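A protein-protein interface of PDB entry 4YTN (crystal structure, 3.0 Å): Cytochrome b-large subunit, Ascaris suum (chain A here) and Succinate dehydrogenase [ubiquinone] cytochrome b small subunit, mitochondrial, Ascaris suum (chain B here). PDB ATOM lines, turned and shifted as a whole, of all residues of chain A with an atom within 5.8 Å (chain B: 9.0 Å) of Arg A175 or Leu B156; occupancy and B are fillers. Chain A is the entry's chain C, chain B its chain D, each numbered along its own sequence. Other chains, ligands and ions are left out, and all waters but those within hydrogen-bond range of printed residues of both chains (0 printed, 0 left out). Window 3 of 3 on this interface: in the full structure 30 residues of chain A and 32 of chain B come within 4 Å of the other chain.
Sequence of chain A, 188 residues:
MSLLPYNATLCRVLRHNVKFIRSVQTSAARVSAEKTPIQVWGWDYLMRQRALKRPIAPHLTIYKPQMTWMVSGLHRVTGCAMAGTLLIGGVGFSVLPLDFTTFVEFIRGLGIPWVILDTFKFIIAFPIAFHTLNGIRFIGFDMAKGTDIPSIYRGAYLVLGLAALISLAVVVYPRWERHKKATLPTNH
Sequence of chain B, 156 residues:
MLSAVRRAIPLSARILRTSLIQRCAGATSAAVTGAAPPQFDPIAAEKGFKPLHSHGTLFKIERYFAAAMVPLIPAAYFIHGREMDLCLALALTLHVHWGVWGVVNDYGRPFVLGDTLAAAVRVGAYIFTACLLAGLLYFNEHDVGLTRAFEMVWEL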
ATOM      1  N   VAL A 104      27.576  12.856 -20.560  1.00  0.00           N
ATOM      2  CA  VAL A 104      27.114  14.231 -20.347  1.00  0.00           C
ATOM      3  C   VAL A 104      27.028  14.544 -18.848  1.00  0.00           C
ATOM      4  O   VAL A 104      27.393  15.643 -18.409  1.00  0.00           O
ATOM      5  CB  VAL A 104      25.753  14.487 -21.035  1.00  0.00           C
ATOM      6  CG1 VAL A 104      25.162  15.833 -20.621  1.00  0.00           C
ATOM      7  CG2 VAL A 104      25.912  14.427 -22.546  1.00  0.00           C
ATOM      8  N   ILE A 107      30.688  15.303 -16.994  1.00  0.00           N
ATOM      9  CA  ILE A 107      31.306  16.640 -17.095  1.00  0.00           C
ATOM     10  C   ILE A 107      30.443  17.718 -16.418  1.00  0.00           C
ATOM     11  O   ILE A 107      30.958  18.751 -15.965  1.00  0.00           O
ATOM     12  CB  ILE A 107      31.649  17.037 -18.561  1.00  0.00           C
ATOM     13  CG1 ILE A 107      30.400  17.472 -19.341  1.00  0.00           C
ATOM     14  CG2 ILE A 107      32.367  15.907 -19.287  1.00  0.00           C
ATOM     15  CD1 ILE A 107      30.140  18.968 -19.310  1.00  0.00           C
ATOM     16  N   ARG A 108      29.132  17.485 -16.362  1.00  0.00           N
ATOM     17  CA  ARG A 108      28.242  18.346 -15.590  1.00  0.00           C
ATOM     18  C   ARG A 108      28.639  18.251 -14.125  1.00  0.00           C
ATOM     19  O   ARG A 108      28.840  19.270 -13.463  1.00  0.00           O
ATOM     20  CB  ARG A 108      26.779  17.941 -15.779  1.00  0.00           C
ATOM     21  CG  ARG A 108      25.796  18.796 -14.988  1.00  0.00           C
ATOM     22  CD  ARG A 108      24.559  19.131 -15.807  1.00  0.00           C
ATOM     23  NE  ARG A 108      23.946  17.935 -16.383  1.00  0.00           N
ATOM     24  CZ  ARG A 108      23.056  17.943 -17.373  1.00  0.00           C
ATOM     25  NH1 ARG A 108      22.571  16.792 -17.819  1.00  0.00           N
ATOM     26  NH2 ARG A 108      22.646  19.083 -17.926  1.00  0.00           N
ATOM     27  N   TRP A 114      30.930  28.502 -16.231  1.00  0.00           N
ATOM     28  CA  TRP A 114      29.917  28.641 -17.285  1.00  0.00           C
ATOM     29  C   TRP A 114      30.507  29.134 -18.610  1.00  0.00           C
ATOM     30  O   TRP A 114      30.140  28.639 -19.677  1.00  0.00           O
ATOM     31  CB  TRP A 114      28.758  29.552 -16.814  1.00  0.00           C
ATOM     32  CG  TRP A 114      28.784  30.991 -17.282  1.00  0.00           C
ATOM     33  CD1 TRP A 114      28.262  31.490 -18.449  1.00  0.00           C
ATOM     34  CD2 TRP A 114      29.330  32.114 -16.577  1.00  0.00           C
ATOM     35  NE1 TRP A 114      28.466  32.848 -18.517  1.00  0.00           N
ATOM     36  CE2 TRP A 114      29.115  33.259 -17.382  1.00  0.00           C
ATOM     37  CE3 TRP A 114      29.989  32.265 -15.345  1.00  0.00           C
ATOM     38  CZ2 TRP A 114      29.540  34.546 -16.994  1.00  0.00           C
ATOM     39  CZ3 TRP A 114      30.411  33.547 -14.957  1.00  0.00           C
ATOM     40  CH2 TRP A 114      30.182  34.667 -15.783  1.00  0.00           C
ATOM     41  N   VAL A 115      31.424  30.098 -18.529  1.00  0.00           N
ATOM     42  CA  VAL A 115      32.032  30.706 -19.716  1.00  0.00           C
ATOM     43  C   VAL A 115      32.849  29.674 -20.473  1.00  0.00           C
ATOM     44  O   VAL A 115      32.792  29.601 -21.701  1.00  0.00           O
ATOM     45  CB  VAL A 115      32.967  31.880 -19.351  1.00  0.00           C
ATOM     46  CG1 VAL A 115      33.622  32.453 -20.604  1.00  0.00           C
ATOM     47  CG2 VAL A 115      32.207  32.965 -18.603  1.00  0.00           C
ATOM     48  N   LEU A 117      32.371  26.506 -20.512  1.00  0.00           N
ATOM     49  CA  LEU A 117      31.464  25.553 -21.163  1.00  0.00           C
ATOM     50  C   LEU A 117      30.899  26.071 -22.486  1.00  0.00           C
ATOM     51  O   LEU A 117      30.661  25.289 -23.403  1.00  0.00           O
ATOM     52  CB  LEU A 117      30.326  25.161 -20.222  1.00  0.00           C
ATOM     53  CG  LEU A 117      30.705  24.058 -19.228  1.00  0.00           C
ATOM     54  CD1 LEU A 117      29.933  24.211 -17.928  1.00  0.00           C
ATOM     55  CD2 LEU A 117      30.466  22.681 -19.831  1.00  0.00           C
ATOM     56  N   ASP A 118      30.682  27.380 -22.580  1.00  0.00           N
ATOM     57  CA  ASP A 118      30.221  28.000 -23.832  1.00  0.00           C
ATOM     58  C   ASP A 118      31.355  28.173 -24.863  1.00  0.00           C
ATOM     59  O   ASP A 118      31.103  28.271 -26.071  1.00  0.00           O
ATOM     60  CB  ASP A 118      29.522  29.335 -23.538  1.00  0.00           C
ATOM     61  CG  ASP A 118      28.103  29.145 -23.014  1.00  0.00           C
ATOM     62  OD1 ASP A 118      27.240  30.014 -23.258  1.00  0.00           O
ATOM     63  OD2 ASP A 118      27.850  28.111 -22.367  1.00  0.00           O
ATOM     64  N   LYS A 121      31.417  24.824 -26.437  1.00  0.00           N
ATOM     65  CA  LYS A 121      30.291  24.812 -27.373  1.00  0.00           C
ATOM     66  C   LYS A 121      30.623  25.562 -28.661  1.00  0.00           C
ATOM     67  O   LYS A 121      30.301  25.102 -29.755  1.00  0.00           O
ATOM     68  CB  LYS A 121      29.051  25.429 -26.729  1.00  0.00           C
ATOM     69  CG  LYS A 121      28.423  24.568 -25.650  1.00  0.00           C
ATOM     70  CD  LYS A 121      27.313  25.308 -24.924  1.00  0.00           C
ATOM     71  CE  LYS A 121      27.006  24.644 -23.596  1.00  0.00           C
ATOM     72  NZ  LYS A 121      25.786  25.198 -22.957  1.00  0.00           N
ATOM     73  N   VAL A 171      25.574  29.894 -29.346  1.00  0.00           N
ATOM     74  CA  VAL A 171      26.092  29.568 -28.015  1.00  0.00           C
ATOM     75  C   VAL A 171      25.585  30.546 -26.962  1.00  0.00           C
ATOM     76  O   VAL A 171      25.419  30.175 -25.799  1.00  0.00           O
ATOM     77  CB  VAL A 171      27.635  29.570 -28.010  1.00  0.00           C
ATOM     78  CG1 VAL A 171      28.196  29.609 -26.596  1.00  0.00           C
ATOM     79  CG2 VAL A 171      28.150  28.347 -28.753  1.00  0.00           C
ATOM     80  N   VAL A 172      25.346  31.790 -27.374  1.00  0.00           N
ATOM     81  CA  VAL A 172      24.984  32.860 -26.448  1.00  0.00           C
ATOM     82  C   VAL A 172      23.463  33.110 -26.389  1.00  0.00           C
ATOM     83  O   VAL A 172      22.978  33.691 -25.424  1.00  0.00           O
ATOM     84  CB  VAL A 172      25.778  34.164 -26.769  1.00  0.00           C
ATOM     85  CG1 VAL A 172      25.008  35.079 -27.720  1.00  0.00           C
ATOM     86  CG2 VAL A 172      26.149  34.905 -25.487  1.00  0.00           C
ATOM     87  N   TYR A 173      22.713  32.670 -27.400  1.00  0.00           N
ATOM     88  CA  TYR A 173      21.258  32.865 -27.412  1.00  0.00           C
ATOM     89  C   TYR A 173      20.526  32.064 -26.335  1.00  0.00           C
ATOM     90  O   TYR A 173      19.655  32.616 -25.662  1.00  0.00           O
ATOM     91  CB  TYR A 173      20.680  32.535 -28.782  1.00  0.00           C
ATOM     92  CG  TYR A 173      19.167  32.518 -28.863  1.00  0.00           C
ATOM     93  CD1 TYR A 173      18.433  33.707 -28.873  1.00  0.00           C
ATOM     94  CD2 TYR A 173      18.469  31.313 -28.970  1.00  0.00           C
ATOM     95  CE1 TYR A 173      17.052  33.694 -28.968  1.00  0.00           C
ATOM     96  CE2 TYR A 173      17.089  31.291 -29.068  1.00  0.00           C
ATOM     97  CZ  TYR A 173      16.386  32.482 -29.067  1.00  0.00           C
ATOM     98  OH  TYR A 173      15.016  32.458 -29.165  1.00  0.00           O
ATOM     99  N   PRO A 174      20.864  30.766 -26.169  1.00  0.00           N
ATOM    100  CA  PRO A 174      20.242  29.992 -25.091  1.00  0.00           C
ATOM    101  C   PRO A 174      20.728  30.414 -23.711  1.00  0.00           C
ATOM    102  O   PRO A 174      19.962  30.349 -22.758  1.00  0.00           O
ATOM    103  CB  PRO A 174      20.671  28.546 -25.374  1.00  0.00           C
ATOM    104  CG  PRO A 174      21.327  28.564 -26.707  1.00  0.00           C
ATOM    105  CD  PRO A 174      21.841  29.954 -26.909  1.00  0.00           C
ATOM    106  N   ARG A 175      21.985  30.842 -23.602  1.00  0.00           N
ATOM    107  CA  ARG A 175      22.521  31.295 -22.320  1.00  0.00           C
ATOM    108  C   ARG A 175      21.934  32.663 -21.911  1.00  0.00           C
ATOM    109  O   ARG A 175      21.903  33.006 -20.724  1.00  0.00           O
ATOM    110  CB  ARG A 175      24.064  31.324 -22.353  1.00  0.00           C
ATOM    111  CG  ARG A 175      24.754  31.107 -21.008  1.00  0.00           C
ATOM    112  CD  ARG A 175      24.015  30.072 -20.172  1.00  0.00           C
ATOM    113  NE  ARG A 175      24.787  29.455 -19.097  1.00  0.00           N
ATOM    114  CZ  ARG A 175      25.727  28.530 -19.271  1.00  0.00           C
ATOM    115  NH1 ARG A 175      26.342  28.010 -18.219  1.00  0.00           N
ATOM    116  NH2 ARG A 175      26.064  28.126 -20.489  1.00  0.00           N
ATOM    117  N   TRP A 176      21.466  33.433 -22.893  1.00  0.00           N
ATOM    118  CA  TRP A 176      20.715  34.663 -22.631  1.00  0.00           C
ATOM    119  C   TRP A 176      19.275  34.288 -22.281  1.00  0.00           C
ATOM    120  O   TRP A 176      18.611  34.989 -21.520  1.00  0.00           O
ATOM    121  CB  TRP A 176      20.748  35.586 -23.860  1.00  0.00           C
ATOM    122  CG  TRP A 176      20.557  37.063 -23.575  1.00  0.00           C
ATOM    123  CD1 TRP A 176      19.608  37.892 -24.117  1.00  0.00           C
ATOM    124  CD2 TRP A 176      21.353  37.881 -22.704  1.00  0.00           C
ATOM    125  NE1 TRP A 176      19.761  39.170 -23.630  1.00  0.00           N
ATOM    126  CE2 TRP A 176      20.822  39.192 -22.761  1.00  0.00           C
ATOM    127  CE3 TRP A 176      22.458  37.633 -21.876  1.00  0.00           C
ATOM    128  CZ2 TRP A 176      21.360  40.251 -22.020  1.00  0.00           C
ATOM    129  CZ3 TRP A 176      22.992  38.688 -21.138  1.00  0.00           C
ATOM    130  CH2 TRP A 176      22.442  39.980 -21.217  1.00  0.00           C
ATOM    131  N   GLU A 177      18.804  33.174 -22.841  1.00  0.00           N
ATOM    132  CA  GLU A 177      17.469  32.649 -22.548  1.00  0.00           C
ATOM    133  C   GLU A 177      17.435  31.847 -21.240  1.00  0.00           C
ATOM    134  O   GLU A 177      16.362  31.613 -20.703  1.00  0.00           O
ATOM    135  CB  GLU A 177      16.961  31.773 -23.707  1.00  0.00           C
ATOM    136  CG  GLU A 177      15.470  31.915 -24.009  1.00  0.00           C
ATOM    137  CD  GLU A 177      15.121  33.179 -24.797  1.00  0.00           C
ATOM    138  OE1 GLU A 177      13.926  33.370 -25.104  1.00  0.00           O
ATOM    139  OE2 GLU A 177      16.026  33.989 -25.112  1.00  0.00           O
ATOM    140  N   ARG A 178      18.597  31.425 -20.738  1.00  0.00           N
ATOM    141  CA  ARG A 178      18.688  30.674 -19.474  1.00  0.00           C
ATOM    142  C   ARG A 178      18.994  31.590 -18.277  1.00  0.00           C
ATOM    143  O   ARG A 178      18.629  31.275 -17.143  1.00  0.00           O
ATOM    144  CB  ARG A 178      19.755  29.581 -19.574  1.00  0.00           C
ATOM    145  CG  ARG A 178      19.538  28.422 -18.614  1.00  0.00           C
ATOM    146  CD  ARG A 178      20.824  27.658 -18.357  1.00  0.00           C
ATOM    147  NE  ARG A 178      21.260  26.889 -19.518  1.00  0.00           N
ATOM    148  CZ  ARG A 178      22.449  26.304 -19.629  1.00  0.00           C
ATOM    149  NH1 ARG A 178      23.351  26.387 -18.656  1.00  0.00           N
ATOM    150  NH2 ARG A 178      22.746  25.630 -20.730  1.00  0.00           N
ATOM    151  N   HIS A 179      19.681  32.702 -18.534  1.00  0.00           N
ATOM    152  CA  HIS A 179      19.860  33.762 -17.534  1.00  0.00           C
ATOM    153  C   HIS A 179      18.582  34.613 -17.423  1.00  0.00           C
ATOM    154  O   HIS A 179      18.397  35.328 -16.437  1.00  0.00           O
ATOM    155  CB  HIS A 179      21.066  34.643 -17.890  1.00  0.00           C
ATOM    156  CG  HIS A 179      21.632  35.395 -16.723  1.00  0.00           C
ATOM    157  ND1 HIS A 179      21.416  36.743 -16.528  1.00  0.00           N
ATOM    158  CD2 HIS A 179      22.406  34.985 -15.691  1.00  0.00           C
ATOM    159  CE1 HIS A 179      22.034  37.131 -15.426  1.00  0.00           C
ATOM    160  NE2 HIS A 179      22.641  36.082 -14.899  1.00  0.00           N
ATOM    161  N   LYS A 180      17.713  34.528 -18.436  1.00  0.00           N
ATOM    162  CA  LYS A 180      16.367  35.129 -18.389  1.00  0.00           C
ATOM    163  C   LYS A 180      15.401  34.382 -17.451  1.00  0.00           C
ATOM    164  O   LYS A 180      14.278  34.834 -17.247  1.00  0.00           O
ATOM    165  CB  LYS A 180      15.738  35.208 -19.797  1.00  0.00           C
ATOM    166  CG  LYS A 180      15.857  36.553 -20.507  1.00  0.00           C
ATOM    167  CD  LYS A 180      14.949  36.596 -21.735  1.00  0.00           C
ATOM    168  CE  LYS A 180      15.231  37.792 -22.638  1.00  0.00           C
ATOM    169  NZ  LYS A 180      16.430  37.605 -23.510  1.00  0.00           N
ATOM    170  N   ALA B 149      21.934  14.267 -28.877  1.00  0.00           N
ATOM    171  CA  ALA B 149      23.262  14.393 -28.259  1.00  0.00           C
ATOM    172  C   ALA B 149      23.769  15.827 -28.306  1.00  0.00           C
ATOM    173  O   ALA B 149      24.490  16.258 -27.408  1.00  0.00           O
ATOM    174  CB  ALA B 149      24.264  13.458 -28.930  1.00  0.00           C
ATOM    175  N   PHE B 150      23.397  16.556 -29.356  1.00  0.00           N
ATOM    176  CA  PHE B 150      23.698  17.982 -29.441  1.00  0.00           C
ATOM    177  C   PHE B 150      22.968  18.809 -28.381  1.00  0.00           C
ATOM    178  O   PHE B 150      23.598  19.598 -27.673  1.00  0.00           O
ATOM    179  CB  PHE B 150      23.397  18.523 -30.837  1.00  0.00           C
ATOM    180  CG  PHE B 150      24.555  18.410 -31.778  1.00  0.00           C
ATOM    181  CD1 PHE B 150      24.475  17.622 -32.916  1.00  0.00           C
ATOM    182  CD2 PHE B 150      25.742  19.083 -31.508  1.00  0.00           C
ATOM    183  CE1 PHE B 150      25.550  17.518 -33.776  1.00  0.00           C
ATOM    184  CE2 PHE B 150      26.820  18.978 -32.361  1.00  0.00           C
ATOM    185  CZ  PHE B 150      26.723  18.194 -33.497  1.00  0.00           C
ATOM    186  N   GLU B 151      21.650  18.640 -28.274  1.00  0.00           N
ATOM    187  CA  GLU B 151      20.884  19.305 -27.220  1.00  0.00           C
ATOM    188  C   GLU B 151      21.590  19.140 -25.879  1.00  0.00           C
ATOM    189  O   GLU B 151      21.861  20.121 -25.180  1.00  0.00           O
ATOM    190  CB  GLU B 151      19.477  18.720 -27.092  1.00  0.00           C
ATOM    191  CG  GLU B 151      18.544  18.989 -28.259  1.00  0.00           C
ATOM    192  CD  GLU B 151      17.215  18.272 -28.107  1.00  0.00           C
ATOM    193  OE1 GLU B 151      16.570  17.991 -29.139  1.00  0.00           O
ATOM    194  OE2 GLU B 151      16.820  17.978 -26.961  1.00  0.00           O
ATOM    195  N   MET B 152      21.909  17.890 -25.550  1.00  0.00           N
ATOM    196  CA  MET B 152      22.409  17.529 -24.221  1.00  0.00           C
ATOM    197  C   MET B 152      23.742  18.170 -23.839  1.00  0.00           C
ATOM    198  O   MET B 152      24.008  18.366 -22.652  1.00  0.00           O
ATOM    199  CB  MET B 152      22.502  16.006 -24.084  1.00  0.00           C
ATOM    200  CG  MET B 152      21.139  15.339 -24.032  1.00  0.00           C
ATOM    201  SD  MET B 152      21.224  13.578 -24.358  1.00  0.00           S
ATOM    202  CE  MET B 152      22.342  13.081 -23.047  1.00  0.00           C
ATOM    203  N   VAL B 153      24.585  18.480 -24.821  1.00  0.00           N
ATOM    204  CA  VAL B 153      25.802  19.248 -24.536  1.00  0.00           C
ATOM    205  C   VAL B 153      25.489  20.744 -24.525  1.00  0.00           C
ATOM    206  O   VAL B 153      26.137  21.510 -23.809  1.00  0.00           O
ATOM    207  CB  VAL B 153      26.976  18.931 -25.490  1.00  0.00           C
ATOM    208  CG1 VAL B 153      27.544  17.555 -25.190  1.00  0.00           C
ATOM    209  CG2 VAL B 153      26.561  19.031 -26.948  1.00  0.00           C
ATOM    210  N   TRP B 154      24.483  21.149 -25.302  1.00  0.00           N
ATOM    211  CA  TRP B 154      24.014  22.537 -25.282  1.00  0.00           C
ATOM    212  C   TRP B 154      23.312  22.911 -23.962  1.00  0.00           C
ATOM    213  O   TRP B 154      23.403  24.061 -23.521  1.00  0.00           O
ATOM    214  CB  TRP B 154      23.136  22.856 -26.509  1.00  0.00           C
ATOM    215  CG  TRP B 154      23.799  23.837 -27.445  1.00  0.00           C
ATOM    216  CD1 TRP B 154      23.448  25.138 -27.641  1.00  0.00           C
ATOM    217  CD2 TRP B 154      24.951  23.605 -28.272  1.00  0.00           C
ATOM    218  NE1 TRP B 154      24.296  25.730 -28.545  1.00  0.00           N
ATOM    219  CE2 TRP B 154      25.226  24.810 -28.951  1.00  0.00           C
ATOM    220  CE3 TRP B 154      25.768  22.496 -28.512  1.00  0.00           C
ATOM    221  CZ2 TRP B 154      26.285  24.935 -29.856  1.00  0.00           C
ATOM    222  CZ3 TRP B 154      26.821  22.623 -29.412  1.00  0.00           C
ATOM    223  CH2 TRP B 154      27.068  23.834 -30.069  1.00  0.00           C
ATOM    224  N   GLU B 155      22.643  21.946 -23.324  1.00  0.00           N
ATOM    225  CA  GLU B 155      21.972  22.171 -22.026  1.00  0.00           C
ATOM    226  C   GLU B 155      22.931  22.421 -20.850  1.00  0.00           C
ATOM    227  O   GLU B 155      22.500  22.868 -19.792  1.00  0.00           O
ATOM    228  CB  GLU B 155      21.069  20.982 -21.674  1.00  0.00           C
ATOM    229  CG  GLU B 155      19.776  20.910 -22.474  1.00  0.00           C
ATOM    230  CD  GLU B 155      19.006  19.621 -22.243  1.00  0.00           C
ATOM    231  OE1 GLU B 155      19.520  18.727 -21.535  1.00  0.00           O
ATOM    232  OE2 GLU B 155      17.884  19.499 -22.777  1.00  0.00           O
ATOM    233  N   LEU B 156      24.217  22.135 -21.033  1.00  0.00           N
ATOM    234  CA  LEU B 156      25.209  22.265 -19.959  1.00  0.00           C
ATOM    235  C   LEU B 156      25.486  23.718 -19.572  1.00  0.00           C
ATOM    236  O   LEU B 156      26.129  23.986 -18.559  1.00  0.00           O
ATOM    237  CB  LEU B 156      26.524  21.611 -20.382  1.00  0.00           C
ATOM    238  CG  LEU B 156      26.487  20.118 -20.706  1.00  0.00           C
ATOM    239  CD1 LEU B 156      27.763  19.731 -21.439  1.00  0.00           C
ATOM    240  CD2 LEU B 156      26.288  19.287 -19.443  1.00  0.00           C
ATOM    241  OXT LEU B 156      25.100  24.664 -20.258  1.00  0.00           O
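The side-chain amino group of Lys A121 lies within hydrogen-bond range of the backbone carbonyl oxygen of Trp B154, at 2.7 Å. The side-chain amino group (NZ) of Lys A121 lies within salt-bridge range of the chain-end carboxylate (OXT) of Leu B156 (2.8 Å). The guanidinium group (NH2) of Arg A175 lies within salt-bridge range of the chain-end carboxylate (OXT) of Leu B156 (3.6 Å). The guanidinium group of Arg A178 lies within hydrogen-bond range of the backbone carbonyl oxygen of Trp B154, at 3.3 Å. The backbone carbonyl oxygen (O) of Glu B155 is in hydrogen-bond range of the guanidinium group (NH2) of Arg A178 (2.9 Å). The guanidinium group of Arg A178 is in salt-bridge range of the chain-end carboxylate of Leu B156 (2.6 Å).
Of the printed residues of chain B, Ile A107 touches Leu B156 (3.3 Å). Tyr A173 touches none of the printed residues of chain B. No residue of chain B comes within 4 Å of Pro A174. Arg A175 touches just one residue of chain B: Leu B156. Of the printed residues of chain A, Met B152 touches Val A104 (3.4 Å). Of the printed residues of chain A, Trp B154 touches Lys A121 (2.7 Å) and Arg A178 (3.3 Å). Of the printed residues of chain A, Glu B155 touches Arg A178 (2.9 Å). Of chain A, only Val A104, Ile A107, Arg A108, Leu A117, Lys A121, Arg A175 and Arg A178 come within 4 Å of Leu B156. The nearest residue of chain B that does not touch Arg A175 is Trp B154 (5.7 Å). The nearest residue of chain A that does not touch Leu B156 is Asp A118 (4.9 Å). The nearest printed residue of chain B that does not touch Arg A108 is Glu B155 (4.2 Å).
NZ of Lys A121 is in salt-bridge range of OD2 of Asp A118, 3.6 Å away. The side-chain carboxylate (OD2) of Asp A118 lies within salt-bridge range of the guanidinium group (NH2) of Arg A175 (2.6 Å).
Met B152 touches Val A104 (O to CG1, 3.4 Å). Val A104 touches Leu B156 (CG1 to CD2, 3.8 Å). Ile A107 touches Leu B156 (CD1 to CD1, 3.3 Å). CB of Arg A108 touches CD2 of Leu B156, 3.9 Å away. Leu A117 touches Leu B156 (CD1 to O, 3.9 Å). Val B153 touches Lys A121 (O to CE, 3.3 Å).
Hydrophobic or aromatic side chains of chain A that line the printed part of chain B: Val A104, Ile A107 and Leu A117. Hydrophobic or aromatic side chains of chain B within 4 Å of the printed part of chain A: Met B152, Trp B154 and Leu B156. Along chain B the printed residues that touch a printed residue of chain A span positions 152 to 156. Among the printed residues, no Asp or Glu carboxylate lies within 4 Å of a Lys or Arg side-chain nitrogen of the other chain.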
